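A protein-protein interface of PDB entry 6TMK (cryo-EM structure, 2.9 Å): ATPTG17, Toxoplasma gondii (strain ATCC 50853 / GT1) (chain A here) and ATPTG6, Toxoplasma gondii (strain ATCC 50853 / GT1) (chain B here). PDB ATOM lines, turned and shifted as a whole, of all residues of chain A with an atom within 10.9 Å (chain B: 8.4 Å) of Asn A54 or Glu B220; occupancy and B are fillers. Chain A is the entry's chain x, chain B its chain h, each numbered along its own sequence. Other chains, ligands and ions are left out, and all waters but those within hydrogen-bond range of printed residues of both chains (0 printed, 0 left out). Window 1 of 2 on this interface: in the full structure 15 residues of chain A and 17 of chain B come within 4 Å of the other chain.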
ATOM      1  N   TRP A  30     -12.975  16.599   4.178  1.00  0.00           N
ATOM      2  CA  TRP A  30     -12.953  18.032   4.427  1.00  0.00           C
ATOM      3  C   TRP A  30     -11.959  18.723   3.508  1.00  0.00           C
ATOM      4  O   TRP A  30     -12.225  19.817   2.995  1.00  0.00           O
ATOM      5  CB  TRP A  30     -12.608  18.302   5.889  1.00  0.00           C
ATOM      6  CG  TRP A  30     -12.428  19.743   6.192  1.00  0.00           C
ATOM      7  CD1 TRP A  30     -11.259  20.382   6.469  1.00  0.00           C
ATOM      8  CD2 TRP A  30     -13.452  20.738   6.241  1.00  0.00           C
ATOM      9  NE1 TRP A  30     -11.489  21.713   6.690  1.00  0.00           N
ATOM     10  CE2 TRP A  30     -12.831  21.959   6.558  1.00  0.00           C
ATOM     11  CE3 TRP A  30     -14.835  20.715   6.050  1.00  0.00           C
ATOM     12  CZ2 TRP A  30     -13.543  23.147   6.686  1.00  0.00           C
ATOM     13  CZ3 TRP A  30     -15.541  21.893   6.179  1.00  0.00           C
ATOM     14  CH2 TRP A  30     -14.895  23.092   6.495  1.00  0.00           C
ATOM     15  N   ARG A  31     -10.805  18.094   3.285  1.00  0.00           N
ATOM     16  CA  ARG A  31      -9.815  18.670   2.386  1.00  0.00           C
ATOM     17  C   ARG A  31     -10.351  18.771   0.969  1.00  0.00           C
ATOM     18  O   ARG A  31     -10.165  19.794   0.298  1.00  0.00           O
ATOM     19  CB  ARG A  31      -8.538  17.840   2.423  1.00  0.00           C
ATOM     20  CG  ARG A  31      -7.728  18.056   3.669  1.00  0.00           C
ATOM     21  CD  ARG A  31      -6.530  17.149   3.714  1.00  0.00           C
ATOM     22  NE  ARG A  31      -5.792  17.294   4.963  1.00  0.00           N
ATOM     23  CZ  ARG A  31      -5.035  16.348   5.502  1.00  0.00           C
ATOM     24  NH1 ARG A  31      -4.897  15.172   4.907  1.00  0.00           N
ATOM     25  NH2 ARG A  31      -4.409  16.586   6.639  1.00  0.00           N
ATOM     26  N   ASN A  34     -12.821  21.681   0.826  1.00  0.00           N
ATOM     27  CA  ASN A  34     -12.139  22.968   0.828  1.00  0.00           C
ATOM     28  C   ASN A  34     -11.503  23.255  -0.526  1.00  0.00           C
ATOM     29  O   ASN A  34     -11.560  24.387  -1.021  1.00  0.00           O
ATOM     30  CB  ASN A  34     -11.094  22.997   1.937  1.00  0.00           C
ATOM     31  CG  ASN A  34     -11.711  23.143   3.311  1.00  0.00           C
ATOM     32  OD1 ASN A  34     -12.890  22.858   3.507  1.00  0.00           O
ATOM     33  ND2 ASN A  34     -10.915  23.595   4.271  1.00  0.00           N
ATOM     34  N   GLY A  35     -10.918  22.235  -1.155  1.00  0.00           N
ATOM     35  CA  GLY A  35     -10.390  22.415  -2.497  1.00  0.00           C
ATOM     36  C   GLY A  35     -11.462  22.749  -3.513  1.00  0.00           C
ATOM     37  O   GLY A  35     -11.270  23.605  -4.381  1.00  0.00           O
ATOM     38  N   THR A  38     -12.487  26.360  -2.972  1.00  0.00           N
ATOM     39  CA  THR A  38     -11.440  27.243  -3.468  1.00  0.00           C
ATOM     40  C   THR A  38     -11.476  27.337  -4.986  1.00  0.00           C
ATOM     41  O   THR A  38     -11.346  28.428  -5.554  1.00  0.00           O
ATOM     42  CB  THR A  38     -10.076  26.742  -2.999  1.00  0.00           C
ATOM     43  OG1 THR A  38     -10.083  26.598  -1.575  1.00  0.00           O
ATOM     44  CG2 THR A  38      -8.986  27.706  -3.407  1.00  0.00           C
ATOM     45  N   GLU A  39     -11.672  26.206  -5.663  1.00  0.00           N
ATOM     46  CA  GLU A  39     -11.688  26.233  -7.119  1.00  0.00           C
ATOM     47  C   GLU A  39     -12.935  26.928  -7.645  1.00  0.00           C
ATOM     48  O   GLU A  39     -12.881  27.620  -8.667  1.00  0.00           O
ATOM     49  CB  GLU A  39     -11.599  24.812  -7.668  1.00  0.00           C
ATOM     50  CG  GLU A  39     -11.384  24.746  -9.167  1.00  0.00           C
ATOM     51  CD  GLU A  39     -10.116  25.451  -9.611  1.00  0.00           C
ATOM     52  OE1 GLU A  39      -9.124  25.424  -8.852  1.00  0.00           O
ATOM     53  OE2 GLU A  39     -10.112  26.032 -10.716  1.00  0.00           O
ATOM     54  N   LYS A  41     -14.464  29.412  -6.110  1.00  0.00           N
ATOM     55  CA  LYS A  41     -14.163  30.827  -5.926  1.00  0.00           C
ATOM     56  C   LYS A  41     -13.251  31.340  -7.033  1.00  0.00           C
ATOM     57  O   LYS A  41     -13.475  32.419  -7.595  1.00  0.00           O
ATOM     58  CB  LYS A  41     -13.536  31.048  -4.553  1.00  0.00           C
ATOM     59  CG  LYS A  41     -13.253  32.491  -4.225  1.00  0.00           C
ATOM     60  CD  LYS A  41     -13.404  32.744  -2.742  1.00  0.00           C
ATOM     61  CE  LYS A  41     -12.510  31.830  -1.931  1.00  0.00           C
ATOM     62  NZ  LYS A  41     -12.294  32.351  -0.554  1.00  0.00           N
ATOM     63  N   THR A  42     -12.210  30.573  -7.356  1.00  0.00           N
ATOM     64  CA  THR A  42     -11.296  30.978  -8.419  1.00  0.00           C
ATOM     65  C   THR A  42     -12.015  31.101  -9.755  1.00  0.00           C
ATOM     66  O   THR A  42     -11.768  32.045 -10.515  1.00  0.00           O
ATOM     67  CB  THR A  42     -10.151  29.976  -8.527  1.00  0.00           C
ATOM     68  OG1 THR A  42      -9.430  29.932  -7.293  1.00  0.00           O
ATOM     69  CG2 THR A  42      -9.220  30.355  -9.644  1.00  0.00           C
ATOM     70  N   LEU A  49      -4.812  36.744  -7.127  1.00  0.00           N
ATOM     71  CA  LEU A  49      -4.870  35.307  -7.313  1.00  0.00           C
ATOM     72  C   LEU A  49      -5.000  34.588  -5.975  1.00  0.00           C
ATOM     73  O   LEU A  49      -4.829  35.165  -4.899  1.00  0.00           O
ATOM     74  CB  LEU A  49      -3.634  34.812  -8.059  1.00  0.00           C
ATOM     75  CG  LEU A  49      -2.262  35.175  -7.499  1.00  0.00           C
ATOM     76  CD1 LEU A  49      -1.804  34.205  -6.436  1.00  0.00           C
ATOM     77  CD2 LEU A  49      -1.261  35.218  -8.623  1.00  0.00           C
ATOM     78  N   LEU A  50      -5.313  33.298  -6.060  1.00  0.00           N
ATOM     79  CA  LEU A  50      -5.312  32.397  -4.920  1.00  0.00           C
ATOM     80  C   LEU A  50      -4.348  31.254  -5.184  1.00  0.00           C
ATOM     81  O   LEU A  50      -4.387  30.636  -6.252  1.00  0.00           O
ATOM     82  CB  LEU A  50      -6.706  31.839  -4.642  1.00  0.00           C
ATOM     83  CG  LEU A  50      -7.808  32.836  -4.297  1.00  0.00           C
ATOM     84  CD1 LEU A  50      -9.107  32.094  -4.121  1.00  0.00           C
ATOM     85  CD2 LEU A  50      -7.472  33.625  -3.050  1.00  0.00           C
ATOM     86  N   TYR A  51      -3.487  30.981  -4.217  1.00  0.00           N
ATOM     87  CA  TYR A  51      -2.641  29.800  -4.275  1.00  0.00           C
ATOM     88  C   TYR A  51      -3.446  28.593  -3.808  1.00  0.00           C
ATOM     89  O   TYR A  51      -3.886  28.568  -2.656  1.00  0.00           O
ATOM     90  CB  TYR A  51      -1.417  29.973  -3.396  1.00  0.00           C
ATOM     91  CG  TYR A  51      -0.484  31.085  -3.796  1.00  0.00           C
ATOM     92  CD1 TYR A  51       0.176  31.060  -5.007  1.00  0.00           C
ATOM     93  CD2 TYR A  51      -0.249  32.153  -2.950  1.00  0.00           C
ATOM     94  CE1 TYR A  51       1.033  32.070  -5.369  1.00  0.00           C
ATOM     95  CE2 TYR A  51       0.604  33.164  -3.305  1.00  0.00           C
ATOM     96  CZ  TYR A  51       1.245  33.119  -4.516  1.00  0.00           C
ATOM     97  OH  TYR A  51       2.100  34.127  -4.880  1.00  0.00           O
ATOM     98  N   PRO A  52      -3.659  27.579  -4.652  1.00  0.00           N
ATOM     99  CA  PRO A  52      -4.587  26.505  -4.277  1.00  0.00           C
ATOM    100  C   PRO A  52      -4.087  25.641  -3.133  1.00  0.00           C
ATOM    101  O   PRO A  52      -4.812  25.407  -2.162  1.00  0.00           O
ATOM    102  CB  PRO A  52      -4.719  25.685  -5.567  1.00  0.00           C
ATOM    103  CG  PRO A  52      -3.993  26.424  -6.612  1.00  0.00           C
ATOM    104  CD  PRO A  52      -3.016  27.303  -5.943  1.00  0.00           C
ATOM    105  N   SER A  53      -2.853  25.159  -3.237  1.00  0.00           N
ATOM    106  CA  SER A  53      -2.303  24.206  -2.288  1.00  0.00           C
ATOM    107  C   SER A  53      -1.644  24.886  -1.101  1.00  0.00           C
ATOM    108  O   SER A  53      -0.819  24.266  -0.422  1.00  0.00           O
ATOM    109  CB  SER A  53      -1.304  23.280  -2.979  1.00  0.00           C
ATOM    110  OG  SER A  53      -1.918  22.526  -4.005  1.00  0.00           O
ATOM    111  N   ASN A  54      -1.990  26.137  -0.834  1.00  0.00           N
ATOM    112  CA  ASN A  54      -1.458  26.868   0.300  1.00  0.00           C
ATOM    113  C   ASN A  54      -2.467  26.901   1.439  1.00  0.00           C
ATOM    114  O   ASN A  54      -3.679  26.810   1.229  1.00  0.00           O
ATOM    115  CB  ASN A  54      -1.095  28.291  -0.115  1.00  0.00           C
ATOM    116  CG  ASN A  54       0.109  28.343  -1.028  1.00  0.00           C
ATOM    117  OD1 ASN A  54       0.253  27.525  -1.934  1.00  0.00           O
ATOM    118  ND2 ASN A  54       0.977  29.315  -0.802  1.00  0.00           N
ATOM    119  N   ARG A  55      -1.942  27.044   2.656  1.00  0.00           N
ATOM    120  CA  ARG A  55      -2.769  26.964   3.854  1.00  0.00           C
ATOM    121  C   ARG A  55      -3.784  28.097   3.912  1.00  0.00           C
ATOM    122  O   ARG A  55      -4.981  27.865   4.113  1.00  0.00           O
ATOM    123  CB  ARG A  55      -1.861  26.982   5.084  1.00  0.00           C
ATOM    124  CG  ARG A  55      -2.548  26.864   6.425  1.00  0.00           C
ATOM    125  CD  ARG A  55      -3.032  25.468   6.696  1.00  0.00           C
ATOM    126  NE  ARG A  55      -4.051  25.454   7.737  1.00  0.00           N
ATOM    127  CZ  ARG A  55      -4.465  24.355   8.354  1.00  0.00           C
ATOM    128  NH1 ARG A  55      -3.952  23.179   8.033  1.00  0.00           N
ATOM    129  NH2 ARG A  55      -5.396  24.434   9.289  1.00  0.00           N
ATOM    130  N   TYR A  56      -3.326  29.332   3.727  1.00  0.00           N
ATOM    131  CA  TYR A  56      -4.151  30.506   3.952  1.00  0.00           C
ATOM    132  C   TYR A  56      -3.844  31.541   2.883  1.00  0.00           C
ATOM    133  O   TYR A  56      -2.684  31.731   2.510  1.00  0.00           O
ATOM    134  CB  TYR A  56      -3.894  31.085   5.350  1.00  0.00           C
ATOM    135  CG  TYR A  56      -4.808  32.211   5.766  1.00  0.00           C
ATOM    136  CD1 TYR A  56      -6.182  32.107   5.631  1.00  0.00           C
ATOM    137  CD2 TYR A  56      -4.296  33.372   6.310  1.00  0.00           C
ATOM    138  CE1 TYR A  56      -7.013  33.132   6.015  1.00  0.00           C
ATOM    139  CE2 TYR A  56      -5.117  34.400   6.699  1.00  0.00           C
ATOM    140  CZ  TYR A  56      -6.475  34.278   6.548  1.00  0.00           C
ATOM    141  OH  TYR A  56      -7.295  35.309   6.937  1.00  0.00           O
ATOM    142  N   ASN A  57      -4.890  32.199   2.384  1.00  0.00           N
ATOM    143  CA  ASN A  57      -4.778  33.195   1.321  1.00  0.00           C
ATOM    144  C   ASN A  57      -5.459  34.474   1.782  1.00  0.00           C
ATOM    145  O   ASN A  57      -6.653  34.679   1.526  1.00  0.00           O
ATOM    146  CB  ASN A  57      -5.399  32.690   0.024  1.00  0.00           C
ATOM    147  CG  ASN A  57      -4.440  31.874  -0.804  1.00  0.00           C
ATOM    148  OD1 ASN A  57      -3.508  32.405  -1.402  1.00  0.00           O
ATOM    149  ND2 ASN A  57      -4.665  30.575  -0.847  1.00  0.00           N
ATOM    150  N   PRO A  58      -4.738  35.364   2.462  1.00  0.00           N
ATOM    151  CA  PRO A  58      -5.355  36.599   2.954  1.00  0.00           C
ATOM    152  C   PRO A  58      -5.379  37.760   1.973  1.00  0.00           C
ATOM    153  O   PRO A  58      -5.907  38.821   2.324  1.00  0.00           O
ATOM    154  CB  PRO A  58      -4.466  36.941   4.151  1.00  0.00           C
ATOM    155  CG  PRO A  58      -3.132  36.440   3.769  1.00  0.00           C
ATOM    156  CD  PRO A  58      -3.338  35.242   2.900  1.00  0.00           C
ATOM    157  N   GLN A  59      -4.844  37.597   0.771  1.00  0.00           N
ATOM    158  CA  GLN A  59      -4.667  38.726  -0.127  1.00  0.00           C
ATOM    159  C   GLN A  59      -6.001  39.266  -0.622  1.00  0.00           C
ATOM    160  O   GLN A  59      -6.902  38.510  -0.994  1.00  0.00           O
ATOM    161  CB  GLN A  59      -3.790  38.334  -1.311  1.00  0.00           C
ATOM    162  CG  GLN A  59      -4.250  37.115  -2.046  1.00  0.00           C
ATOM    163  CD  GLN A  59      -3.538  35.869  -1.601  1.00  0.00           C
ATOM    164  OE1 GLN A  59      -2.974  35.813  -0.513  1.00  0.00           O
ATOM    165  NE2 GLN A  59      -3.568  34.855  -2.439  1.00  0.00           N
ATOM    166  N   ARG A  65      -0.134  39.329   0.160  1.00  0.00           N
ATOM    167  CA  ARG A  65      -0.147  37.876   0.213  1.00  0.00           C
ATOM    168  C   ARG A  65       0.540  37.320   1.448  1.00  0.00           C
ATOM    169  O   ARG A  65       0.741  36.106   1.529  1.00  0.00           O
ATOM    170  CB  ARG A  65       0.507  37.310  -1.042  1.00  0.00           C
ATOM    171  CG  ARG A  65      -0.235  37.653  -2.294  1.00  0.00           C
ATOM    172  CD  ARG A  65       0.449  37.149  -3.529  1.00  0.00           C
ATOM    173  NE  ARG A  65      -0.145  37.718  -4.731  1.00  0.00           N
ATOM    174  CZ  ARG A  65       0.321  37.527  -5.957  1.00  0.00           C
ATOM    175  NH1 ARG A  65       1.389  36.778  -6.151  1.00  0.00           N
ATOM    176  NH2 ARG A  65      -0.282  38.089  -6.990  1.00  0.00           N
ATOM    177  N   MET A  66       0.909  38.172   2.405  1.00  0.00           N
ATOM    178  CA  MET A  66       1.431  37.715   3.687  1.00  0.00           C
ATOM    179  C   MET A  66       0.711  38.376   4.852  1.00  0.00           C
ATOM    180  O   MET A  66       1.207  38.341   5.981  1.00  0.00           O
ATOM    181  CB  MET A  66       2.932  37.974   3.787  1.00  0.00           C
ATOM    182  CG  MET A  66       3.751  37.337   2.691  1.00  0.00           C
ATOM    183  SD  MET A  66       3.595  35.546   2.620  1.00  0.00           S
ATOM    184  CE  MET A  66       4.459  35.076   4.106  1.00  0.00           C
ATOM    185  N   ASN B 217       5.507  35.470  -2.165  1.00  0.00           N
ATOM    186  CA  ASN B 217       5.122  34.106  -1.871  1.00  0.00           C
ATOM    187  C   ASN B 217       5.370  33.272  -3.113  1.00  0.00           C
ATOM    188  O   ASN B 217       5.779  33.782  -4.158  1.00  0.00           O
ATOM    189  CB  ASN B 217       3.664  34.034  -1.424  1.00  0.00           C
ATOM    190  CG  ASN B 217       3.392  32.862  -0.528  1.00  0.00           C
ATOM    191  OD1 ASN B 217       3.964  31.790  -0.697  1.00  0.00           O
ATOM    192  ND2 ASN B 217       2.512  33.054   0.432  1.00  0.00           N
ATOM    193  N   TYR B 218       5.124  31.979  -2.988  1.00  0.00           N
ATOM    194  CA  TYR B 218       5.385  31.045  -4.065  1.00  0.00           C
ATOM    195  C   TYR B 218       4.275  30.013  -4.122  1.00  0.00           C
ATOM    196  O   TYR B 218       3.596  29.749  -3.129  1.00  0.00           O
ATOM    197  CB  TYR B 218       6.744  30.357  -3.898  1.00  0.00           C
ATOM    198  CG  TYR B 218       6.909  29.596  -2.614  1.00  0.00           C
ATOM    199  CD1 TYR B 218       6.725  28.231  -2.573  1.00  0.00           C
ATOM    200  CD2 TYR B 218       7.257  30.242  -1.444  1.00  0.00           C
ATOM    201  CE1 TYR B 218       6.876  27.534  -1.408  1.00  0.00           C
ATOM    202  CE2 TYR B 218       7.407  29.554  -0.280  1.00  0.00           C
ATOM    203  CZ  TYR B 218       7.214  28.200  -0.261  1.00  0.00           C
ATOM    204  OH  TYR B 218       7.370  27.509   0.915  1.00  0.00           O
ATOM    205  N   ILE B 219       4.089  29.447  -5.310  1.00  0.00           N
ATOM    206  CA  ILE B 219       3.095  28.402  -5.510  1.00  0.00           C
ATOM    207  C   ILE B 219       3.628  27.136  -4.850  1.00  0.00           C
ATOM    208  O   ILE B 219       4.615  26.556  -5.309  1.00  0.00           O
ATOM    209  CB  ILE B 219       2.803  28.177  -6.995  1.00  0.00           C
ATOM    210  CG1 ILE B 219       2.091  29.378  -7.593  1.00  0.00           C
ATOM    211  CG2 ILE B 219       1.933  26.981  -7.183  1.00  0.00           C
ATOM    212  CD1 ILE B 219       2.355  29.544  -9.043  1.00  0.00           C
ATOM    213  N   GLU B 220       2.990  26.712  -3.769  1.00  0.00           N
ATOM    214  CA  GLU B 220       3.334  25.451  -3.139  1.00  0.00           C
ATOM    215  C   GLU B 220       2.730  24.291  -3.914  1.00  0.00           C
ATOM    216  O   GLU B 220       1.618  24.386  -4.439  1.00  0.00           O
ATOM    217  CB  GLU B 220       2.847  25.426  -1.694  1.00  0.00           C
ATOM    218  CG  GLU B 220       3.692  26.241  -0.754  1.00  0.00           C
ATOM    219  CD  GLU B 220       3.306  26.044   0.693  1.00  0.00           C
ATOM    220  OE1 GLU B 220       2.725  24.986   1.014  1.00  0.00           O
ATOM    221  OE2 GLU B 220       3.582  26.947   1.510  1.00  0.00           O
ATOM    222  N   ASP B 221       3.471  23.190  -3.981  1.00  0.00           N
ATOM    223  CA  ASP B 221       2.999  22.019  -4.690  1.00  0.00           C
ATOM    224  C   ASP B 221       1.996  21.248  -3.846  1.00  0.00           C
ATOM    225  O   ASP B 221       1.881  21.435  -2.633  1.00  0.00           O
ATOM    226  CB  ASP B 221       4.161  21.108  -5.069  1.00  0.00           C
ATOM    227  CG  ASP B 221       3.787  20.105  -6.144  1.00  0.00           C
ATOM    228  OD1 ASP B 221       2.696  20.244  -6.736  1.00  0.00           O
ATOM    229  OD2 ASP B 221       4.577  19.173  -6.392  1.00  0.00           O
ATOM    230  N   ARG B 222       1.259  20.370  -4.514  1.00  0.00           N
ATOM    231  CA  ARG B 222       0.319  19.518  -3.819  1.00  0.00           C
ATOM    232  C   ARG B 222       1.045  18.638  -2.809  1.00  0.00           C
ATOM    233  O   ARG B 222       2.266  18.479  -2.831  1.00  0.00           O
ATOM    234  CB  ARG B 222      -0.446  18.655  -4.813  1.00  0.00           C
ATOM    235  CG  ARG B 222      -1.276  19.433  -5.793  1.00  0.00           C
ATOM    236  CD  ARG B 222      -1.696  18.566  -6.941  1.00  0.00           C
ATOM    237  NE  ARG B 222      -2.760  17.643  -6.569  1.00  0.00           N
ATOM    238  CZ  ARG B 222      -2.936  16.448  -7.119  1.00  0.00           C
ATOM    239  NH1 ARG B 222      -2.118  16.018  -8.067  1.00  0.00           N
ATOM    240  NH2 ARG B 222      -3.931  15.678  -6.711  1.00  0.00           N
ATOM    241  N   ARG B 223       0.258  18.050  -1.922  1.00  0.00           N
ATOM    242  CA  ARG B 223       0.812  17.237  -0.858  1.00  0.00           C
ATOM    243  C   ARG B 223       1.369  15.939  -1.421  1.00  0.00           C
ATOM    244  O   ARG B 223       0.815  15.360  -2.358  1.00  0.00           O
ATOM    245  CB  ARG B 223      -0.258  16.968   0.188  1.00  0.00           C
ATOM    246  CG  ARG B 223       0.286  16.608   1.530  1.00  0.00           C
ATOM    247  CD  ARG B 223      -0.806  16.548   2.563  1.00  0.00           C
ATOM    248  NE  ARG B 223      -0.496  15.611   3.631  1.00  0.00           N
ATOM    249  CZ  ARG B 223      -0.951  15.727   4.871  1.00  0.00           C
ATOM    250  NH1 ARG B 223      -1.739  16.739   5.205  1.00  0.00           N
ATOM    251  NH2 ARG B 223      -0.611  14.832   5.781  1.00  0.00           N
ATOM    252  N   GLN B 237       0.020  20.192  11.332  1.00  0.00           N
ATOM    253  CA  GLN B 237      -0.066  21.219  10.311  1.00  0.00           C
ATOM    254  C   GLN B 237       0.873  22.369  10.638  1.00  0.00           C
ATOM    255  O   GLN B 237       0.914  22.852  11.773  1.00  0.00           O
ATOM    256  CB  GLN B 237      -1.498  21.727  10.192  1.00  0.00           C
ATOM    257  CG  GLN B 237      -2.482  20.678   9.748  1.00  0.00           C
ATOM    258  CD  GLN B 237      -2.296  20.270   8.309  1.00  0.00           C
ATOM    259  OE1 GLN B 237      -2.559  21.045   7.391  1.00  0.00           O
ATOM    260  NE2 GLN B 237      -1.849  19.042   8.101  1.00  0.00           N
ATOM    261  N   TYR B 238       1.628  22.797   9.634  1.00  0.00           N
ATOM    262  CA  TYR B 238       2.584  23.883   9.750  1.00  0.00           C
ATOM    263  C   TYR B 238       2.216  24.976   8.760  1.00  0.00           C
ATOM    264  O   TYR B 238       1.820  24.698   7.625  1.00  0.00           O
ATOM    265  CB  TYR B 238       4.006  23.388   9.515  1.00  0.00           C
ATOM    266  CG  TYR B 238       4.474  22.436  10.585  1.00  0.00           C
ATOM    267  CD1 TYR B 238       4.624  22.862  11.893  1.00  0.00           C
ATOM    268  CD2 TYR B 238       4.741  21.111  10.299  1.00  0.00           C
ATOM    269  CE1 TYR B 238       5.039  22.003  12.878  1.00  0.00           C
ATOM    270  CE2 TYR B 238       5.158  20.243  11.281  1.00  0.00           C
ATOM    271  CZ  TYR B 238       5.299  20.694  12.569  1.00  0.00           C
ATOM    272  OH  TYR B 238       5.714  19.832  13.553  1.00  0.00           O
ATOM    273  N   SER B 239       2.346  26.216   9.210  1.00  0.00           N
ATOM    274  CA  SER B 239       1.966  27.382   8.432  1.00  0.00           C
ATOM    275  C   SER B 239       2.697  27.439   7.096  1.00  0.00           C
ATOM    276  O   SER B 239       2.179  27.978   6.118  1.00  0.00           O
ATOM    277  CB  SER B 239       2.255  28.641   9.242  1.00  0.00           C
ATOM    278  OG  SER B 239       1.637  28.567  10.512  1.00  0.00           O
ATOM    279  OXT SER B 239       3.816  26.945   6.960  1.00  0.00           O
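Of the printed residues of chain B, Arg A31 touches Arg B223 (3.0 Å) and Gln B237 (3.8 Å).
Of chain B, only Asn B217 (3.9 Å), Tyr B218 (3.5 Å) and Glu B220 (3.3 Å) come within 4 Å of Asn A54.
Printed residues of chain B within 4 Å of Arg A65: Asn B217.
Of chain A, only Asn A54 (3.5 Å) comes within 4 Å of Tyr B218.
Of chain A, only Ser A53 (3.7 Å) comes within 4 Å of Asp B221.
Of the printed residues of chain A, Arg B222 touches Ser A53 (3.6 Å).
The nearest residue of chain A that does not touch Glu B220 is Tyr A51 (5.3 Å).
The nearest printed residue of chain A that does not touch Arg B223 is Ser A53 (5.4 Å).
The backbone NH (N) of Glu B220 lies close to the side-chain amide oxygen (OD1) of Asn A54 (3.4 Å).
The guanidinium group of Arg A31 lies close to the guanidinium group of Arg B223, at 3.0 Å.
The side-chain amide oxygen of Gln B237 is in hydrogen-bond range of the guanidinium group of Arg A55.
ND2 of Asn B217 lies within hydrogen-bond range of SD of Met A66 (3.5 Å).
Of the 10 printed residues of chain B, 8 touch a printed residue of chain A.
Hydrophobic or aromatic side chains of chain B that line the printed part of chain A: Ile B219.
Among the printed residues, no Asp or Glu carboxylate lies within 4 Å of a Lys or Arg side-chain nitrogen of the other chain.
OH of Tyr A51 is in hydrogen-bond range of NH1 of Arg A65.
O of Tyr A51 lies within hydrogen-bond range of ND2 of Asn A57 (2.8 Å).
Arg A31 touches Gln B237 (NH2 to NE2, 3.8 Å).
Asn B217 touches Tyr A51.
Ile B219 touches Tyr A51.
CB of Ser A53 touches O of Glu B220 (3.4 Å).
CB of Ser A53 touches O of Asp B221, 3.7 Å away.
OG of Ser A53 touches CG of Arg B222 (3.6 Å).
OD1 of Asn B217 touches ND2 of Asn A54, 3.9 Å away.
Tyr B218 touches Asn A54.
Arg A65 touches Asn B217 (O to ND2, 3.7 Å).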
